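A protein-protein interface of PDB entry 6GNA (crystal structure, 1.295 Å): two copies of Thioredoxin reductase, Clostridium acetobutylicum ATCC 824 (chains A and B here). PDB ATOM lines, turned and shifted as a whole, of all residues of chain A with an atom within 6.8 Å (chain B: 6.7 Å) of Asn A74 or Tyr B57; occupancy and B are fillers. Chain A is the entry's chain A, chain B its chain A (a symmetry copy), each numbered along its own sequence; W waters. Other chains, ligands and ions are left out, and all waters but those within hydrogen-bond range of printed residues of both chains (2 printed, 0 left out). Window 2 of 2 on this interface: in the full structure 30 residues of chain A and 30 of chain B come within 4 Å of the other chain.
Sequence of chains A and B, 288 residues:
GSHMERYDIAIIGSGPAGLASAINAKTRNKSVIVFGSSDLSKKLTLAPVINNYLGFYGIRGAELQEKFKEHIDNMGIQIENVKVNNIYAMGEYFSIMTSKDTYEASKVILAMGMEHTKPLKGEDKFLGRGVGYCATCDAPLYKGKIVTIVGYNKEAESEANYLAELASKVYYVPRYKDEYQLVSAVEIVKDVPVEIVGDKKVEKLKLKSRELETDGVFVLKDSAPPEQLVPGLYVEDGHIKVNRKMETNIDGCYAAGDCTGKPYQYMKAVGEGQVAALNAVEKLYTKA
Printed residues of chain B within 4 Å of Lys A67: Gly B55 (3.9 Å).
Lys A69 touches none of the printed residues of chain B.
Of chain B, only Tyr B57 (3.6 Å) comes within 4 Å of Asn A74.
Val B49 touches none of the printed residues of chain A.
Printed residues of chain A within 4 Å of Gly B55: Lys A67 and His A71.
Tyr B57 touches just these residues of chain A: His A71 (3.6 Å), Asn A74 (3.6 Å) and Met A75 (3.6 Å).
The nearest printed residue of chain A that does not touch Leu B54 is Ile A72 (4.8 Å).
No position is printed for both chains.
N of Gly B58 sits at hydrogen-bond distance from OD1 of Asn B51 (3.0 Å).
The backbone carbonyl oxygen (O) of Glu A70 sits close to the side-chain amide oxygen (OD1) of Asn A74 (3.1 Å).
The side-chain sulfur of Met A75 sits close to a ring nitrogen (ND1) of His A71 (3.6 Å).
Lys A67 touches Gly B55.
His A71 touches Leu B54.
His A71 touches Gly B55 (CD2 to N, 3.1 Å).
His A71 touches Phe B56 (CD2 to N, 3.8 Å).
Tyr B57 touches His A71 (N to CD2, 3.6 Å).
Asn A74 touches Tyr B57.
Tyr B57 touches Met A75.
Of the 10 printed residues of chain A, 4 touch a printed residue of chain B.
Printed residues of chain A that touch a printed residue of chain B: Lys A67, His A71, Asn A74 and Met A75.
Hydrophobic or aromatic side chains of chain A that line the printed part of chain B: His A71 and Met A75.
Among the printed residues, no Asp or Glu carboxylate lies within 4 Å of a Lys or Arg side-chain nitrogen of the other chain.
NE2 of His A71 lies within hydrogen-bond range of O of Tyr B53 (3.4 Å).
O of Asn B51 sits close to NE2 of His A71 (3.2 Å).
The side-chain sulfur (SD) of Met A75 sits close to the backbone carbonyl oxygen (O) of Asn B51.
Water W2 lies within hydrogen-bond range of the backbone carbonyl oxygen of Ile B50 (2.8 Å), the backbone NH of Tyr B53 (2.9 Å), the backbone carbonyl oxygen of Phe B56 (3.0 Å), the backbone NH of Asn B52 (3.3 Å) and a ring nitrogen (NE2) of His A71 (3.5 Å).
Water W1 lies within hydrogen-bond range of the backbone carbonyl oxygen of Lys A67 (3.2 Å), the backbone carbonyl oxygen of Gly B55 (3.2 Å) and the backbone NH of Tyr B57 (3.3 Å).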
ATOM      1  N   LYS A  67     -26.697 -15.333 -20.723  1.00  0.00           N
ATOM      2  CA  LYS A  67     -26.014 -16.464 -21.335  1.00  0.00           C
ATOM      3  C   LYS A  67     -24.503 -16.265 -21.277  1.00  0.00           C
ATOM      4  O   LYS A  67     -23.750 -17.219 -21.032  1.00  0.00           O
ATOM      5  CB  LYS A  67     -26.459 -16.628 -22.792  1.00  0.00           C
ATOM      6  CG  LYS A  67     -27.979 -16.825 -22.990  1.00  0.00           C
ATOM      7  CD  LYS A  67     -28.368 -18.259 -22.911  1.00  0.00           C
ATOM      8  CE  LYS A  67     -29.793 -18.478 -23.383  1.00  0.00           C
ATOM      9  NZ  LYS A  67     -30.311 -19.705 -22.763  1.00  0.00           N
ATOM     10  N   LYS A  69     -22.832 -14.410 -19.068  1.00  0.00           N
ATOM     11  CA  LYS A  69     -22.435 -14.541 -17.673  1.00  0.00           C
ATOM     12  C   LYS A  69     -22.323 -16.007 -17.263  1.00  0.00           C
ATOM     13  O   LYS A  69     -21.374 -16.401 -16.574  1.00  0.00           O
ATOM     14  CB  LYS A  69     -23.434 -13.798 -16.793  1.00  0.00           C
ATOM     15  CG  LYS A  69     -23.078 -13.788 -15.327  1.00  0.00           C
ATOM     16  CD  LYS A  69     -21.661 -13.315 -15.074  1.00  0.00           C
ATOM     17  CE  LYS A  69     -21.459 -12.901 -13.624  1.00  0.00           C
ATOM     18  NZ  LYS A  69     -22.005 -13.905 -12.668  1.00  0.00           N
ATOM     19  N   GLU A  70     -23.286 -16.830 -17.662  1.00  0.00           N
ATOM     20  CA  GLU A  70     -23.225 -18.229 -17.263  1.00  0.00           C
ATOM     21  C   GLU A  70     -22.053 -18.933 -17.928  1.00  0.00           C
ATOM     22  O   GLU A  70     -21.416 -19.795 -17.310  1.00  0.00           O
ATOM     23  CB  GLU A  70     -24.558 -18.900 -17.569  1.00  0.00           C
ATOM     24  CG  GLU A  70     -25.654 -18.319 -16.694  1.00  0.00           C
ATOM     25  CD  GLU A  70     -26.954 -19.078 -16.764  1.00  0.00           C
ATOM     26  OE1 GLU A  70     -26.945 -20.261 -17.164  1.00  0.00           O
ATOM     27  OE2 GLU A  70     -27.986 -18.475 -16.412  1.00  0.00           O
ATOM     28  N   HIS A  71     -21.711 -18.533 -19.159  1.00  0.00           N
ATOM     29  CA  HIS A  71     -20.560 -19.114 -19.834  1.00  0.00           C
ATOM     30  C   HIS A  71     -19.284 -18.851 -19.045  1.00  0.00           C
ATOM     31  O   HIS A  71     -18.526 -19.778 -18.746  1.00  0.00           O
ATOM     32  CB  HIS A  71     -20.455 -18.502 -21.229  1.00  0.00           C
ATOM     33  CG  HIS A  71     -19.659 -19.312 -22.197  1.00  0.00           C
ATOM     34  ND1 HIS A  71     -18.460 -19.916 -21.886  1.00  0.00           N
ATOM     35  CD2 HIS A  71     -19.889 -19.590 -23.496  1.00  0.00           C
ATOM     36  CE1 HIS A  71     -18.005 -20.553 -22.950  1.00  0.00           C
ATOM     37  NE2 HIS A  71     -18.856 -20.368 -23.935  1.00  0.00           N
ATOM     38  N   ILE A  72     -19.018 -17.586 -18.703  1.00  0.00           N
ATOM     39  CA  ILE A  72     -17.755 -17.302 -18.026  1.00  0.00           C
ATOM     40  C   ILE A  72     -17.739 -17.936 -16.643  1.00  0.00           C
ATOM     41  O   ILE A  72     -16.703 -18.438 -16.193  1.00  0.00           O
ATOM     42  CB  ILE A  72     -17.407 -15.798 -18.015  1.00  0.00           C
ATOM     43  CG1 ILE A  72     -18.446 -14.955 -17.276  1.00  0.00           C
ATOM     44  CG2 ILE A  72     -17.226 -15.307 -19.444  1.00  0.00           C
ATOM     45  CD1 ILE A  72     -17.987 -13.504 -17.078  1.00  0.00           C
ATOM     46  N   ASP A  73     -18.884 -17.942 -15.962  1.00  0.00           N
ATOM     47  CA  ASP A  73     -18.977 -18.594 -14.662  1.00  0.00           C
ATOM     48  C   ASP A  73     -18.680 -20.086 -14.776  1.00  0.00           C
ATOM     49  O   ASP A  73     -17.934 -20.641 -13.962  1.00  0.00           O
ATOM     50  CB  ASP A  73     -20.365 -18.358 -14.069  1.00  0.00           C
ATOM     51  CG  ASP A  73     -20.596 -16.899 -13.674  1.00  0.00           C
ATOM     52  OD1 ASP A  73     -19.633 -16.097 -13.701  1.00  0.00           O
ATOM     53  OD2 ASP A  73     -21.749 -16.556 -13.338  1.00  0.00           O
ATOM     54  N   ASN A  74     -19.227 -20.751 -15.798  1.00  0.00           N
ATOM     55  CA  ASN A  74     -18.915 -22.158 -15.994  1.00  0.00           C
ATOM     56  C   ASN A  74     -17.427 -22.396 -16.231  1.00  0.00           C
ATOM     57  O   ASN A  74     -16.928 -23.487 -15.936  1.00  0.00           O
ATOM     58  CB  ASN A  74     -19.718 -22.730 -17.164  1.00  0.00           C
ATOM     59  CG  ASN A  74     -21.097 -23.215 -16.747  1.00  0.00           C
ATOM     60  OD1 ASN A  74     -22.111 -22.819 -17.321  1.00  0.00           O
ATOM     61  ND2 ASN A  74     -21.136 -24.086 -15.748  1.00  0.00           N
ATOM     62  N   MET A  75     -16.708 -21.428 -16.797  1.00  0.00           N
ATOM     63  CA  MET A  75     -15.283 -21.587 -17.054  1.00  0.00           C
ATOM     64  C   MET A  75     -14.401 -20.964 -15.978  1.00  0.00           C
ATOM     65  O   MET A  75     -13.187 -20.854 -16.181  1.00  0.00           O
ATOM     66  CB  MET A  75     -14.930 -20.999 -18.412  1.00  0.00           C
ATOM     67  CG  MET A  75     -15.612 -21.742 -19.529  1.00  0.00           C
ATOM     68  SD  MET A  75     -15.176 -21.139 -21.154  1.00  0.00           S
ATOM     69  CE  MET A  75     -13.564 -21.884 -21.371  1.00  0.00           C
ATOM     70  N   GLY A  76     -14.972 -20.551 -14.855  1.00  0.00           N
ATOM     71  CA  GLY A  76     -14.163 -20.016 -13.777  1.00  0.00           C
ATOM     72  C   GLY A  76     -13.494 -18.701 -14.102  1.00  0.00           C
ATOM     73  O   GLY A  76     -12.414 -18.415 -13.581  1.00  0.00           O
ATOM     74  N   ILE A  77     -14.095 -17.904 -14.979  1.00  0.00           N
ATOM     75  CA  ILE A  77     -13.581 -16.594 -15.356  1.00  0.00           C
ATOM     76  C   ILE A  77     -14.342 -15.564 -14.549  1.00  0.00           C
ATOM     77  O   ILE A  77     -15.571 -15.493 -14.632  1.00  0.00           O
ATOM     78  CB  ILE A  77     -13.789 -16.343 -16.854  1.00  0.00           C
ATOM     79  CG1 ILE A  77     -12.892 -17.276 -17.658  1.00  0.00           C
ATOM     80  CG2 ILE A  77     -13.520 -14.879 -17.210  1.00  0.00           C
ATOM     81  CD1 ILE A  77     -13.243 -17.361 -19.121  1.00  0.00           C
ATOM     82  N   VAL B  49     -18.173 -31.564 -28.099  1.00  0.00           N
ATOM     83  CA  VAL B  49     -18.589 -30.500 -27.197  1.00  0.00           C
ATOM     84  C   VAL B  49     -17.864 -29.228 -27.612  1.00  0.00           C
ATOM     85  O   VAL B  49     -16.678 -29.271 -27.942  1.00  0.00           O
ATOM     86  CB  VAL B  49     -18.277 -30.873 -25.741  1.00  0.00           C
ATOM     87  CG1 VAL B  49     -16.787 -31.136 -25.569  1.00  0.00           C
ATOM     88  CG2 VAL B  49     -18.760 -29.778 -24.792  1.00  0.00           C
ATOM     89  N   ILE B  50     -18.569 -28.096 -27.591  1.00  0.00           N
ATOM     90  CA  ILE B  50     -18.010 -26.802 -27.980  1.00  0.00           C
ATOM     91  C   ILE B  50     -18.110 -25.877 -26.781  1.00  0.00           C
ATOM     92  O   ILE B  50     -19.215 -25.599 -26.298  1.00  0.00           O
ATOM     93  CB  ILE B  50     -18.757 -26.198 -29.176  1.00  0.00           C
ATOM     94  CG1 ILE B  50     -18.676 -27.142 -30.374  1.00  0.00           C
ATOM     95  CG2 ILE B  50     -18.218 -24.795 -29.513  1.00  0.00           C
ATOM     96  CD1 ILE B  50     -19.722 -26.867 -31.412  1.00  0.00           C
ATOM     97  N   ASN B  51     -16.967 -25.384 -26.315  1.00  0.00           N
ATOM     98  CA  ASN B  51     -16.924 -24.491 -25.166  1.00  0.00           C
ATOM     99  C   ASN B  51     -16.411 -23.098 -25.480  1.00  0.00           C
ATOM    100  O   ASN B  51     -16.327 -22.275 -24.568  1.00  0.00           O
ATOM    101  CB  ASN B  51     -16.082 -25.100 -24.038  1.00  0.00           C
ATOM    102  CG  ASN B  51     -16.661 -26.391 -23.531  1.00  0.00           C
ATOM    103  OD1 ASN B  51     -17.878 -26.530 -23.434  1.00  0.00           O
ATOM    104  ND2 ASN B  51     -15.800 -27.343 -23.200  1.00  0.00           N
ATOM    105  N   ASN B  52     -16.077 -22.800 -26.732  1.00  0.00           N
ATOM    106  CA  ASN B  52     -15.539 -21.497 -27.091  1.00  0.00           C
ATOM    107  C   ASN B  52     -16.443 -20.752 -28.058  1.00  0.00           C
ATOM    108  O   ASN B  52     -15.958 -19.901 -28.812  1.00  0.00           O
ATOM    109  CB  ASN B  52     -14.121 -21.632 -27.643  1.00  0.00           C
ATOM    110  CG  ASN B  52     -14.085 -22.324 -28.980  1.00  0.00           C
ATOM    111  OD1 ASN B  52     -15.079 -22.879 -29.429  1.00  0.00           O
ATOM    112  ND2 ASN B  52     -12.931 -22.258 -29.649  1.00  0.00           N
ATOM    113  N   TYR B  53     -17.728 -21.053 -28.068  1.00  0.00           N
ATOM    114  CA  TYR B  53     -18.722 -20.236 -28.752  1.00  0.00           C
ATOM    115  C   TYR B  53     -19.543 -19.531 -27.674  1.00  0.00           C
ATOM    116  O   TYR B  53     -20.387 -20.151 -27.014  1.00  0.00           O
ATOM    117  CB  TYR B  53     -19.573 -21.078 -29.695  1.00  0.00           C
ATOM    118  CG  TYR B  53     -20.403 -20.256 -30.648  1.00  0.00           C
ATOM    119  CD1 TYR B  53     -19.895 -19.834 -31.842  1.00  0.00           C
ATOM    120  CD2 TYR B  53     -21.737 -19.964 -30.368  1.00  0.00           C
ATOM    121  CE1 TYR B  53     -20.649 -19.078 -32.724  1.00  0.00           C
ATOM    122  CE2 TYR B  53     -22.518 -19.199 -31.249  1.00  0.00           C
ATOM    123  CZ  TYR B  53     -21.943 -18.762 -32.446  1.00  0.00           C
ATOM    124  OH  TYR B  53     -22.586 -18.005 -33.416  1.00  0.00           O
ATOM    125  N   LEU B  54     -19.306 -18.227 -27.542  1.00  0.00           N
ATOM    126  CA  LEU B  54     -19.757 -17.466 -26.383  1.00  0.00           C
ATOM    127  C   LEU B  54     -21.280 -17.458 -26.300  1.00  0.00           C
ATOM    128  O   LEU B  54     -21.974 -17.072 -27.250  1.00  0.00           O
ATOM    129  CB  LEU B  54     -19.221 -16.043 -26.459  1.00  0.00           C
ATOM    130  CG  LEU B  54     -19.527 -15.163 -25.235  1.00  0.00           C
ATOM    131  CD1 LEU B  54     -18.876 -15.681 -23.947  1.00  0.00           C
ATOM    132  CD2 LEU B  54     -19.119 -13.726 -25.511  1.00  0.00           C
ATOM    133  N   GLY B  55     -21.792 -17.861 -25.147  1.00  0.00           N
ATOM    134  CA  GLY B  55     -23.212 -17.999 -24.920  1.00  0.00           C
ATOM    135  C   GLY B  55     -23.750 -19.410 -25.028  1.00  0.00           C
ATOM    136  O   GLY B  55     -24.889 -19.651 -24.600  1.00  0.00           O
ATOM    137  N   PHE B  56     -22.973 -20.350 -25.564  1.00  0.00           N
ATOM    138  CA  PHE B  56     -23.403 -21.737 -25.747  1.00  0.00           C
ATOM    139  C   PHE B  56     -22.443 -22.715 -25.081  1.00  0.00           C
ATOM    140  O   PHE B  56     -22.085 -23.746 -25.644  1.00  0.00           O
ATOM    141  CB  PHE B  56     -23.526 -22.097 -27.225  1.00  0.00           C
ATOM    142  CG  PHE B  56     -24.722 -21.509 -27.921  1.00  0.00           C
ATOM    143  CD1 PHE B  56     -26.004 -21.935 -27.629  1.00  0.00           C
ATOM    144  CD2 PHE B  56     -24.553 -20.564 -28.906  1.00  0.00           C
ATOM    145  CE1 PHE B  56     -27.087 -21.396 -28.300  1.00  0.00           C
ATOM    146  CE2 PHE B  56     -25.617 -20.033 -29.577  1.00  0.00           C
ATOM    147  CZ  PHE B  56     -26.880 -20.439 -29.280  1.00  0.00           C
ATOM    148  N   TYR B  57     -21.995 -22.423 -23.873  1.00  0.00           N
ATOM    149  CA  TYR B  57     -21.063 -23.330 -23.212  1.00  0.00           C
ATOM    150  C   TYR B  57     -21.606 -24.752 -23.149  1.00  0.00           C
ATOM    151  O   TYR B  57     -22.757 -24.982 -22.756  1.00  0.00           O
ATOM    152  CB  TYR B  57     -20.779 -22.829 -21.798  1.00  0.00           C
ATOM    153  CG  TYR B  57     -19.884 -23.756 -21.018  1.00  0.00           C
ATOM    154  CD1 TYR B  57     -18.513 -23.706 -21.175  1.00  0.00           C
ATOM    155  CD2 TYR B  57     -20.412 -24.691 -20.134  1.00  0.00           C
ATOM    156  CE1 TYR B  57     -17.678 -24.551 -20.459  1.00  0.00           C
ATOM    157  CE2 TYR B  57     -19.590 -25.544 -19.422  1.00  0.00           C
ATOM    158  CZ  TYR B  57     -18.221 -25.471 -19.595  1.00  0.00           C
ATOM    159  OH  TYR B  57     -17.396 -26.320 -18.898  1.00  0.00           O
ATOM    160  N   GLY B  58     -20.758 -25.711 -23.528  1.00  0.00           N
ATOM    161  CA  GLY B  58     -21.085 -27.119 -23.396  1.00  0.00           C
ATOM    162  C   GLY B  58     -22.002 -27.664 -24.462  1.00  0.00           C
ATOM    163  O   GLY B  58     -22.444 -28.819 -24.354  1.00  0.00           O
ATOM    164  N   ILE B  59     -22.303 -26.879 -25.492  1.00  0.00           N
ATOM    165  CA  ILE B  59     -23.200 -27.346 -26.539  1.00  0.00           C
ATOM    166  C   ILE B  59     -22.496 -28.377 -27.412  1.00  0.00           C
ATOM    167  O   ILE B  59     -21.278 -28.341 -27.615  1.00  0.00           O
ATOM    168  CB  ILE B  59     -23.698 -26.138 -27.355  1.00  0.00           C
ATOM    169  CG1 ILE B  59     -24.896 -26.525 -28.211  1.00  0.00           C
ATOM    170  CG2 ILE B  59     -22.584 -25.546 -28.229  1.00  0.00           C
ATOM    171  CD1 ILE B  59     -25.640 -25.320 -28.718  1.00  0.00           C
HETATM  172  O   HOH W   1     -23.421 -20.252 -21.860  1.00  0.00           O
HETATM  173  O   HOH W   2     -19.332 -22.757 -26.429  1.00  0.00           O
